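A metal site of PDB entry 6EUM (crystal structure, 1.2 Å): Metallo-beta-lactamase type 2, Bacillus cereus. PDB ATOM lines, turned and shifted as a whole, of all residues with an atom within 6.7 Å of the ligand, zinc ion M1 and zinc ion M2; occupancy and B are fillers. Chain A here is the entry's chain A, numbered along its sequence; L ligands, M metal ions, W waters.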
ATOM      1  N   PHE A  34     -25.830  33.857 -22.716  1.00  0.00           N
ATOM      2  CA  PHE A  34     -24.544  33.400 -23.234  1.00  0.00           C
ATOM      3  C   PHE A  34     -24.431  33.798 -24.702  1.00  0.00           C
ATOM      4  O   PHE A  34     -25.014  33.150 -25.589  1.00  0.00           O
ATOM      5  CB  PHE A  34     -24.403  31.896 -23.041  1.00  0.00           C
ATOM      6  CG  PHE A  34     -24.431  31.501 -21.595  1.00  0.00           C
ATOM      7  CD1 PHE A  34     -23.266  31.458 -20.853  1.00  0.00           C
ATOM      8  CD2 PHE A  34     -25.630  31.206 -20.979  1.00  0.00           C
ATOM      9  CE1 PHE A  34     -23.280  31.105 -19.526  1.00  0.00           C
ATOM     10  CE2 PHE A  34     -25.660  30.852 -19.663  1.00  0.00           C
ATOM     11  CZ  PHE A  34     -24.482  30.804 -18.922  1.00  0.00           C
ATOM     12  N   VAL A  39     -30.496  31.018 -22.034  1.00  0.00           N
ATOM     13  CA  VAL A  39     -30.509  29.573 -21.861  1.00  0.00           C
ATOM     14  C   VAL A  39     -31.132  29.311 -20.491  1.00  0.00           C
ATOM     15  O   VAL A  39     -30.521  29.597 -19.448  1.00  0.00           O
ATOM     16  CB  VAL A  39     -29.095  29.001 -21.886  1.00  0.00           C
ATOM     17  CG1 VAL A  39     -29.145  27.524 -21.784  1.00  0.00           C
ATOM     18  CG2 VAL A  39     -28.360  29.472 -23.180  1.00  0.00           C
ATOM     19  N   SER A  41     -32.489  27.231 -17.175  1.00  0.00           N
ATOM     20  CA  SER A  41     -32.189  26.022 -16.441  1.00  0.00           C
ATOM     21  C   SER A  41     -33.075  25.914 -15.203  1.00  0.00           C
ATOM     22  O   SER A  41     -33.421  26.928 -14.583  1.00  0.00           O
ATOM     23  CB  SER A  41     -30.719  25.968 -16.031  1.00  0.00           C
ATOM     24  OG  SER A  41     -30.475  26.975 -15.108  1.00  0.00           O
ATOM     25  N   TRP A  59     -26.768  29.650 -12.544  1.00  0.00           N
ATOM     26  CA  TRP A  59     -25.581  29.854 -13.401  1.00  0.00           C
ATOM     27  C   TRP A  59     -24.492  30.633 -12.740  1.00  0.00           C
ATOM     28  O   TRP A  59     -23.320  30.484 -13.146  1.00  0.00           O
ATOM     29  CB  TRP A  59     -26.032  30.644 -14.648  1.00  0.00           C
ATOM     30  CG  TRP A  59     -27.010  29.931 -15.524  1.00  0.00           C
ATOM     31  CD1 TRP A  59     -28.401  30.114 -15.578  1.00  0.00           C
ATOM     32  CD2 TRP A  59     -26.703  28.967 -16.533  1.00  0.00           C
ATOM     33  NE1 TRP A  59     -28.922  29.330 -16.556  1.00  0.00           N
ATOM     34  CE2 TRP A  59     -27.912  28.579 -17.150  1.00  0.00           C
ATOM     35  CE3 TRP A  59     -25.508  28.379 -16.959  1.00  0.00           C
ATOM     36  CZ2 TRP A  59     -27.943  27.677 -18.226  1.00  0.00           C
ATOM     37  CZ3 TRP A  59     -25.556  27.491 -18.044  1.00  0.00           C
ATOM     38  CH2 TRP A  59     -26.768  27.106 -18.620  1.00  0.00           C
ATOM     39  N   HIS A  86     -24.603  18.094 -10.321  1.00  0.00           N
ATOM     40  CA  HIS A  86     -23.328  17.840 -11.017  1.00  0.00           C
ATOM     41  C   HIS A  86     -22.530  19.126 -10.983  1.00  0.00           C
ATOM     42  O   HIS A  86     -23.010  20.159 -10.527  1.00  0.00           O
ATOM     43  CB  HIS A  86     -23.423  17.242 -12.415  1.00  0.00           C
ATOM     44  CG  HIS A  86     -24.020  18.067 -13.488  1.00  0.00           C
ATOM     45  ND1 HIS A  86     -25.365  18.223 -13.669  1.00  0.00           N
ATOM     46  CD2 HIS A  86     -23.440  18.693 -14.543  1.00  0.00           C
ATOM     47  CE1 HIS A  86     -25.573  18.961 -14.755  1.00  0.00           C
ATOM     48  NE2 HIS A  86     -24.426  19.267 -15.309  1.00  0.00           N
ATOM     49  N   ALA A  87     -21.295  19.061 -11.455  1.00  0.00           N
ATOM     50  CA  ALA A  87     -20.333  20.173 -11.319  1.00  0.00           C
ATOM     51  C   ALA A  87     -20.230  21.062 -12.566  1.00  0.00           C
ATOM     52  O   ALA A  87     -19.239  21.865 -12.594  1.00  0.00           O
ATOM     53  CB  ALA A  87     -18.948  19.639 -10.961  1.00  0.00           C
ATOM     54  N   HIS A  88     -21.291  21.324 -13.276  1.00  0.00           N
ATOM     55  CA  HIS A  88     -21.360  22.369 -14.312  1.00  0.00           C
ATOM     56  C   HIS A  88     -21.974  23.677 -13.730  1.00  0.00           C
ATOM     57  O   HIS A  88     -22.747  23.657 -12.769  1.00  0.00           O
ATOM     58  CB  HIS A  88     -22.198  21.915 -15.514  1.00  0.00           C
ATOM     59  CG  HIS A  88     -21.511  20.938 -16.413  1.00  0.00           C
ATOM     60  ND1 HIS A  88     -22.257  20.153 -17.297  1.00  0.00           N
ATOM     61  CD2 HIS A  88     -20.193  20.703 -16.691  1.00  0.00           C
ATOM     62  CE1 HIS A  88     -21.383  19.535 -18.056  1.00  0.00           C
ATOM     63  NE2 HIS A  88     -20.152  19.809 -17.712  1.00  0.00           N
ATOM     64  N   ALA A  89     -21.764  24.799 -14.426  1.00  0.00           N
ATOM     65  CA  ALA A  89     -22.121  26.124 -13.933  1.00  0.00           C
ATOM     66  C   ALA A  89     -23.623  26.264 -13.659  1.00  0.00           C
ATOM     67  O   ALA A  89     -23.984  26.974 -12.723  1.00  0.00           O
ATOM     68  CB  ALA A  89     -21.678  27.202 -14.920  1.00  0.00           C
ATOM     69  N   ASP A  90     -24.498  25.662 -14.478  1.00  0.00           N
ATOM     70  CA  ASP A  90     -25.940  25.803 -14.225  1.00  0.00           C
ATOM     71  C   ASP A  90     -26.323  25.249 -12.867  1.00  0.00           C
ATOM     72  O   ASP A  90     -27.299  25.733 -12.277  1.00  0.00           O
ATOM     73  CB  ASP A  90     -26.775  25.173 -15.386  1.00  0.00           C
ATOM     74  CG  ASP A  90     -26.589  23.696 -15.640  1.00  0.00           C
ATOM     75  OD1 ASP A  90     -25.458  23.191 -15.369  1.00  0.00           O
ATOM     76  OD2 ASP A  90     -27.548  22.988 -16.116  1.00  0.00           O
ATOM     77  N   ARG A  91     -25.657  24.211 -12.381  1.00  0.00           N
ATOM     78  CA  ARG A  91     -25.953  23.561 -11.118  1.00  0.00           C
ATOM     79  C   ARG A  91     -25.251  24.220  -9.952  1.00  0.00           C
ATOM     80  O   ARG A  91     -25.828  24.413  -8.879  1.00  0.00           O
ATOM     81  CB  ARG A  91     -25.492  22.132 -11.192  1.00  0.00           C
ATOM     82  CG  ARG A  91     -25.995  21.313 -12.367  1.00  0.00           C
ATOM     83  CD  ARG A  91     -27.476  21.022 -12.407  1.00  0.00           C
ATOM     84  NE  ARG A  91     -28.145  21.861 -13.405  1.00  0.00           N
ATOM     85  CZ  ARG A  91     -29.433  22.095 -13.454  1.00  0.00           C
ATOM     86  NH1 ARG A  91     -30.221  21.606 -12.525  1.00  0.00           N
ATOM     87  NH2 ARG A  91     -29.922  22.716 -14.465  1.00  0.00           N
ATOM     88  N   TYR A 120     -14.181  25.826  -8.773  1.00  0.00           N
ATOM     89  CA  TYR A 120     -15.275  26.214  -7.901  1.00  0.00           C
ATOM     90  C   TYR A 120     -15.002  25.859  -6.445  1.00  0.00           C
ATOM     91  O   TYR A 120     -14.282  24.893  -6.142  1.00  0.00           O
ATOM     92  CB  TYR A 120     -16.544  25.455  -8.352  1.00  0.00           C
ATOM     93  CG  TYR A 120     -17.161  25.942  -9.641  1.00  0.00           C
ATOM     94  CD1 TYR A 120     -17.702  27.202  -9.736  1.00  0.00           C
ATOM     95  CD2 TYR A 120     -17.256  25.095 -10.749  1.00  0.00           C
ATOM     96  CE1 TYR A 120     -18.257  27.661 -10.898  1.00  0.00           C
ATOM     97  CE2 TYR A 120     -17.807  25.524 -11.973  1.00  0.00           C
ATOM     98  CZ  TYR A 120     -18.297  26.823 -12.055  1.00  0.00           C
ATOM     99  OH  TYR A 120     -18.853  27.235 -13.250  1.00  0.00           O
ATOM    100  N   HIS A 149     -24.816  12.444 -18.855  1.00  0.00           N
ATOM    101  CA  HIS A 149     -24.493  13.795 -19.252  1.00  0.00           C
ATOM    102  C   HIS A 149     -23.127  14.256 -18.736  1.00  0.00           C
ATOM    103  O   HIS A 149     -22.385  14.893 -19.468  1.00  0.00           O
ATOM    104  CB  HIS A 149     -25.602  14.725 -18.752  1.00  0.00           C
ATOM    105  CG  HIS A 149     -25.263  16.161 -18.765  1.00  0.00           C
ATOM    106  ND1 HIS A 149     -25.148  16.884 -19.912  1.00  0.00           N
ATOM    107  CD2 HIS A 149     -24.931  17.003 -17.752  1.00  0.00           C
ATOM    108  CE1 HIS A 149     -24.811  18.133 -19.616  1.00  0.00           C
ATOM    109  NE2 HIS A 149     -24.627  18.261 -18.302  1.00  0.00           N
ATOM    110  N   THR A 150     -22.797  13.822 -17.518  1.00  0.00           N
ATOM    111  CA  THR A 150     -21.469  13.956 -16.966  1.00  0.00           C
ATOM    112  C   THR A 150     -21.164  12.702 -16.201  1.00  0.00           C
ATOM    113  O   THR A 150     -22.005  11.830 -15.996  1.00  0.00           O
ATOM    114  CB  THR A 150     -21.322  15.135 -15.993  1.00  0.00           C
ATOM    115  OG1 THR A 150     -22.269  14.970 -14.954  1.00  0.00           O
ATOM    116  CG2 THR A 150     -21.477  16.445 -16.680  1.00  0.00           C
ATOM    117  N   GLY A 167     -32.538  16.324 -13.683  1.00  0.00           N
ATOM    118  CA  GLY A 167     -31.399  17.155 -13.927  1.00  0.00           C
ATOM    119  C   GLY A 167     -30.971  16.956 -15.364  1.00  0.00           C
ATOM    120  O   GLY A 167     -31.728  16.594 -16.266  1.00  0.00           O
ATOM    121  N   CSO A 168     -29.683  17.182 -15.632  1.00  0.00           N
ATOM    122  CA  CSO A 168     -29.251  17.285 -17.012  1.00  0.00           C
ATOM    123  CB  CSO A 168     -28.148  18.287 -17.150  1.00  0.00           C
ATOM    124  SG  CSO A 168     -28.550  19.867 -16.241  1.00  0.00           S
ATOM    125  C   CSO A 168     -29.000  15.916 -17.655  1.00  0.00           C
ATOM    126  O   CSO A 168     -28.807  15.854 -18.874  1.00  0.00           O
ATOM    127  N   LEU A 169     -29.110  14.859 -16.876  1.00  0.00           N
ATOM    128  CA  LEU A 169     -29.218  13.496 -17.399  1.00  0.00           C
ATOM    129  C   LEU A 169     -30.431  13.313 -18.281  1.00  0.00           C
ATOM    130  O   LEU A 169     -30.462  12.410 -19.131  1.00  0.00           O
ATOM    131  CB  LEU A 169     -29.273  12.515 -16.187  1.00  0.00           C
ATOM    132  CG  LEU A 169     -29.300  11.046 -16.498  1.00  0.00           C
ATOM    133  CD1 LEU A 169     -27.925  10.548 -16.949  1.00  0.00           C
ATOM    134  CD2 LEU A 169     -29.775  10.281 -15.247  1.00  0.00           C
ATOM    135  N   LYS A 171     -33.257  14.829 -20.909  1.00  0.00           N
ATOM    136  CA  LYS A 171     -33.604  15.849 -21.862  1.00  0.00           C
ATOM    137  C   LYS A 171     -35.103  16.100 -21.915  1.00  0.00           C
ATOM    138  O   LYS A 171     -35.925  15.178 -21.832  1.00  0.00           O
ATOM    139  CB  LYS A 171     -33.107  15.467 -23.251  1.00  0.00           C
ATOM    140  CG  LYS A 171     -31.597  15.091 -23.304  1.00  0.00           C
ATOM    141  CD  LYS A 171     -30.639  16.083 -22.819  1.00  0.00           C
ATOM    142  CE  LYS A 171     -30.527  17.272 -23.567  1.00  0.00           C
ATOM    143  NZ  LYS A 171     -29.395  18.175 -23.037  1.00  0.00           N
ATOM    144  N   LEU A 178     -28.415  15.835 -27.919  1.00  0.00           N
ATOM    145  CA  LEU A 178     -27.927  15.665 -26.569  1.00  0.00           C
ATOM    146  C   LEU A 178     -27.283  16.906 -25.990  1.00  0.00           C
ATOM    147  O   LEU A 178     -26.960  16.900 -24.778  1.00  0.00           O
ATOM    148  CB  LEU A 178     -26.939  14.507 -26.531  1.00  0.00           C
ATOM    149  CG  LEU A 178     -27.582  13.164 -26.864  1.00  0.00           C
ATOM    150  CD1 LEU A 178     -26.420  12.167 -27.072  1.00  0.00           C
ATOM    151  CD2 LEU A 178     -28.503  12.752 -25.746  1.00  0.00           C
ATOM    152  N   GLY A 179     -27.090  17.943 -26.787  1.00  0.00           N
ATOM    153  CA  GLY A 179     -26.447  19.137 -26.317  1.00  0.00           C
ATOM    154  C   GLY A 179     -24.938  18.970 -26.170  1.00  0.00           C
ATOM    155  O   GLY A 179     -24.294  18.261 -26.935  1.00  0.00           O
ATOM    156  N   ASN A 180     -24.356  19.630 -25.189  1.00  0.00           N
ATOM    157  CA  ASN A 180     -22.918  19.600 -25.048  1.00  0.00           C
ATOM    158  C   ASN A 180     -22.510  18.263 -24.442  1.00  0.00           C
ATOM    159  O   ASN A 180     -22.855  17.942 -23.302  1.00  0.00           O
ATOM    160  CB  ASN A 180     -22.479  20.772 -24.179  1.00  0.00           C
ATOM    161  CG  ASN A 180     -20.988  20.950 -24.149  1.00  0.00           C
ATOM    162  OD1 ASN A 180     -20.298  20.005 -24.005  1.00  0.00           O
ATOM    163  ND2 ASN A 180     -20.499  22.174 -24.260  1.00  0.00           N
ATOM    164  N   VAL A 181     -21.750  17.501 -25.219  1.00  0.00           N
ATOM    165  CA  VAL A 181     -21.329  16.172 -24.822  1.00  0.00           C
ATOM    166  C   VAL A 181     -19.813  16.117 -24.578  1.00  0.00           C
ATOM    167  O   VAL A 181     -19.256  15.004 -24.366  1.00  0.00           O
ATOM    168  CB  VAL A 181     -21.776  15.113 -25.831  1.00  0.00           C
ATOM    169  CG1 VAL A 181     -23.290  15.003 -25.847  1.00  0.00           C
ATOM    170  CG2 VAL A 181     -21.245  15.480 -27.268  1.00  0.00           C
ATOM    171  N   ALA A 182     -19.190  17.256 -24.356  1.00  0.00           N
ATOM    172  CA  ALA A 182     -17.765  17.231 -24.063  1.00  0.00           C
ATOM    173  C   ALA A 182     -17.433  16.425 -22.833  1.00  0.00           C
ATOM    174  O   ALA A 182     -16.406  15.728 -22.801  1.00  0.00           O
ATOM    175  CB  ALA A 182     -17.230  18.643 -23.880  1.00  0.00           C
ATOM    176  N   ASP A 183     -18.266  16.478 -21.799  1.00  0.00           N
ATOM    177  CA  ASP A 183     -18.048  15.797 -20.563  1.00  0.00           C
ATOM    178  C   ASP A 183     -18.933  14.583 -20.405  1.00  0.00           C
ATOM    179  O   ASP A 183     -18.973  14.001 -19.307  1.00  0.00           O
ATOM    180  CB  ASP A 183     -18.282  16.767 -19.407  1.00  0.00           C
ATOM    181  CG  ASP A 183     -17.330  17.957 -19.408  1.00  0.00           C
ATOM    182  OD1 ASP A 183     -16.181  17.804 -19.796  1.00  0.00           O
ATOM    183  OD2 ASP A 183     -17.761  19.044 -18.956  1.00  0.00           O
ATOM    184  N   GLY A 209     -33.224  19.029 -16.544  1.00  0.00           N
ATOM    185  CA  GLY A 209     -32.346  20.137 -16.217  1.00  0.00           C
ATOM    186  C   GLY A 209     -32.683  21.435 -16.953  1.00  0.00           C
ATOM    187  O   GLY A 209     -32.433  22.535 -16.458  1.00  0.00           O
ATOM    188  N   HIS A 210     -33.202  21.303 -18.167  1.00  0.00           N
ATOM    189  CA  HIS A 210     -33.568  22.398 -19.036  1.00  0.00           C
ATOM    190  C   HIS A 210     -34.886  22.006 -19.706  1.00  0.00           C
ATOM    191  O   HIS A 210     -35.009  20.896 -20.198  1.00  0.00           O
ATOM    192  CB  HIS A 210     -32.436  22.682 -20.109  1.00  0.00           C
ATOM    193  CG  HIS A 210     -31.063  22.825 -19.460  1.00  0.00           C
ATOM    194  ND1 HIS A 210     -30.557  24.004 -18.960  1.00  0.00           N
ATOM    195  CD2 HIS A 210     -30.109  21.896 -19.173  1.00  0.00           C
ATOM    196  CE1 HIS A 210     -29.367  23.769 -18.418  1.00  0.00           C
ATOM    197  NE2 HIS A 210     -29.062  22.502 -18.531  1.00  0.00           N
HETATM  198  C1  LIG L   1     -21.972  21.971 -20.274  1.00  0.00           C
HETATM  199  C2  LIG L   1     -20.809  22.549 -19.816  1.00  0.00           C
HETATM  200  C3  LIG L   1     -20.899  23.749 -19.123  1.00  0.00           C
HETATM  201  C4  LIG L   1     -22.135  24.336 -18.950  1.00  0.00           C
HETATM  202  C5  LIG L   1     -23.279  23.756 -19.438  1.00  0.00           C
HETATM  203  C6  LIG L   1     -26.593  20.685 -20.325  1.00  0.00           C
HETATM  204  O1  LIG L   1     -27.435  20.262 -19.463  1.00  0.00           O
HETATM  205  C7  LIG L   1     -25.440  21.437 -19.764  1.00  0.00           C
HETATM  206  C8  LIG L   1     -24.441  21.821 -20.593  1.00  0.00           C
HETATM  207  C9  LIG L   1     -23.244  22.536 -20.118  1.00  0.00           C
HETATM  208  F1  LIG L   1     -21.900  20.770 -20.902  1.00  0.00           F
HETATM  209  F2  LIG L   1     -24.437  24.429 -19.337  1.00  0.00           F
HETATM  210  F3  LIG L   1     -22.237  25.518 -18.293  1.00  0.00           F
HETATM  211  O2  LIG L   1     -26.671  20.381 -21.500  1.00  0.00           O
HETATM  212  S1  LIG L   1     -25.367  21.767 -17.983  1.00  0.00           S
HETATM  213 ZN    ZN M   1     -24.191  19.890 -17.222  1.00  0.00          ZN
HETATM  214 ZN    ZN M   2     -27.597  21.489 -17.514  1.00  0.00          ZN
HETATM  215  O   HOH W   1     -29.248  18.302 -20.297  1.00  0.00           O
HETATM  216  O   HOH W   2     -25.847  21.400 -23.781  1.00  0.00           O
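An oxygen (O2) of the ligand is in salt-bridge range of the side-chain amino group (NZ) of Lys 171, 3.8 Å away.
A ring nitrogen (NE2) of His 88 sits at hydrogen-bond distance from the side-chain carboxylate (OD2) of Asp 183, 2.8 Å away.
NE of Arg 91 is in salt-bridge range of OD1 of Asp 90 (3.6 Å).
SG of CSO 168 lies close to NE of Arg 91, 3.5 Å away.
The side-chain amide oxygen (OD1) of Asn 180 sits at hydrogen-bond distance from the backbone NH (N) of Ala 182 (3.0 Å).
The indole nitrogen of Trp 59 is in hydrogen-bond range of the side-chain hydroxyl of Ser 41, at 3.2 Å.
The indole nitrogen (NE1) of Trp 59 sits at hydrogen-bond distance from the backbone carbonyl oxygen (O) of Val 39.
The backbone carbonyl oxygen of Leu 178 is in hydrogen-bond range of the side-chain amino group of Lys 171, 3.3 Å away.
Trp 59 touches the ligand.
CB of Ala 89 touches F3 of the ligand, at 3.8 Å.
Asn 180 touches the ligand (CB to F1, 3.3 Å).
Within 4 Å of the ligand: Trp 59, His 86, His 88, Ala 89, Asp 90, His 149, CSO 168, Lys 171, Asn 180 and His 210.
Along chain A the residues within 4 Å of the ligand span positions 59 to 210.
Of the 25 residues printed, 3 come within 4 Å of zinc ion M2.
A ring nitrogen (ND1) of His 88 binds zinc ion M1.
Zinc ion M1 is bound by NE2 of His 149 (2.0 Å).
NE2 of His 86 binds zinc ion M1.
Zinc ion M1 is bound by S1 of the ligand (2.3 Å).
Zinc ion M1 has four donor atoms within binding distance.
The side-chain carboxylate (OD2) of Asp 90 binds zinc ion M2, at 2.1 Å.
Zinc ion M2 is bound by a ring nitrogen (NE2) of His 210, at 2.1 Å.
SG of CSO 168 is bound to zinc ion M2, at 2.3 Å.
A sulfur (S1) of the ligand is bound to zinc ion M2 (2.3 Å).
Zinc ion M2 is bound by an oxygen (O1) of the ligand, 2.3 Å away.
Water W2 bridges O2 of the ligand and N of Asn 180.
Water W1 bridges the side-chain amino group (NZ) of Lys 171 (2.7 Å) and O of CSO 168 (2.9 Å).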
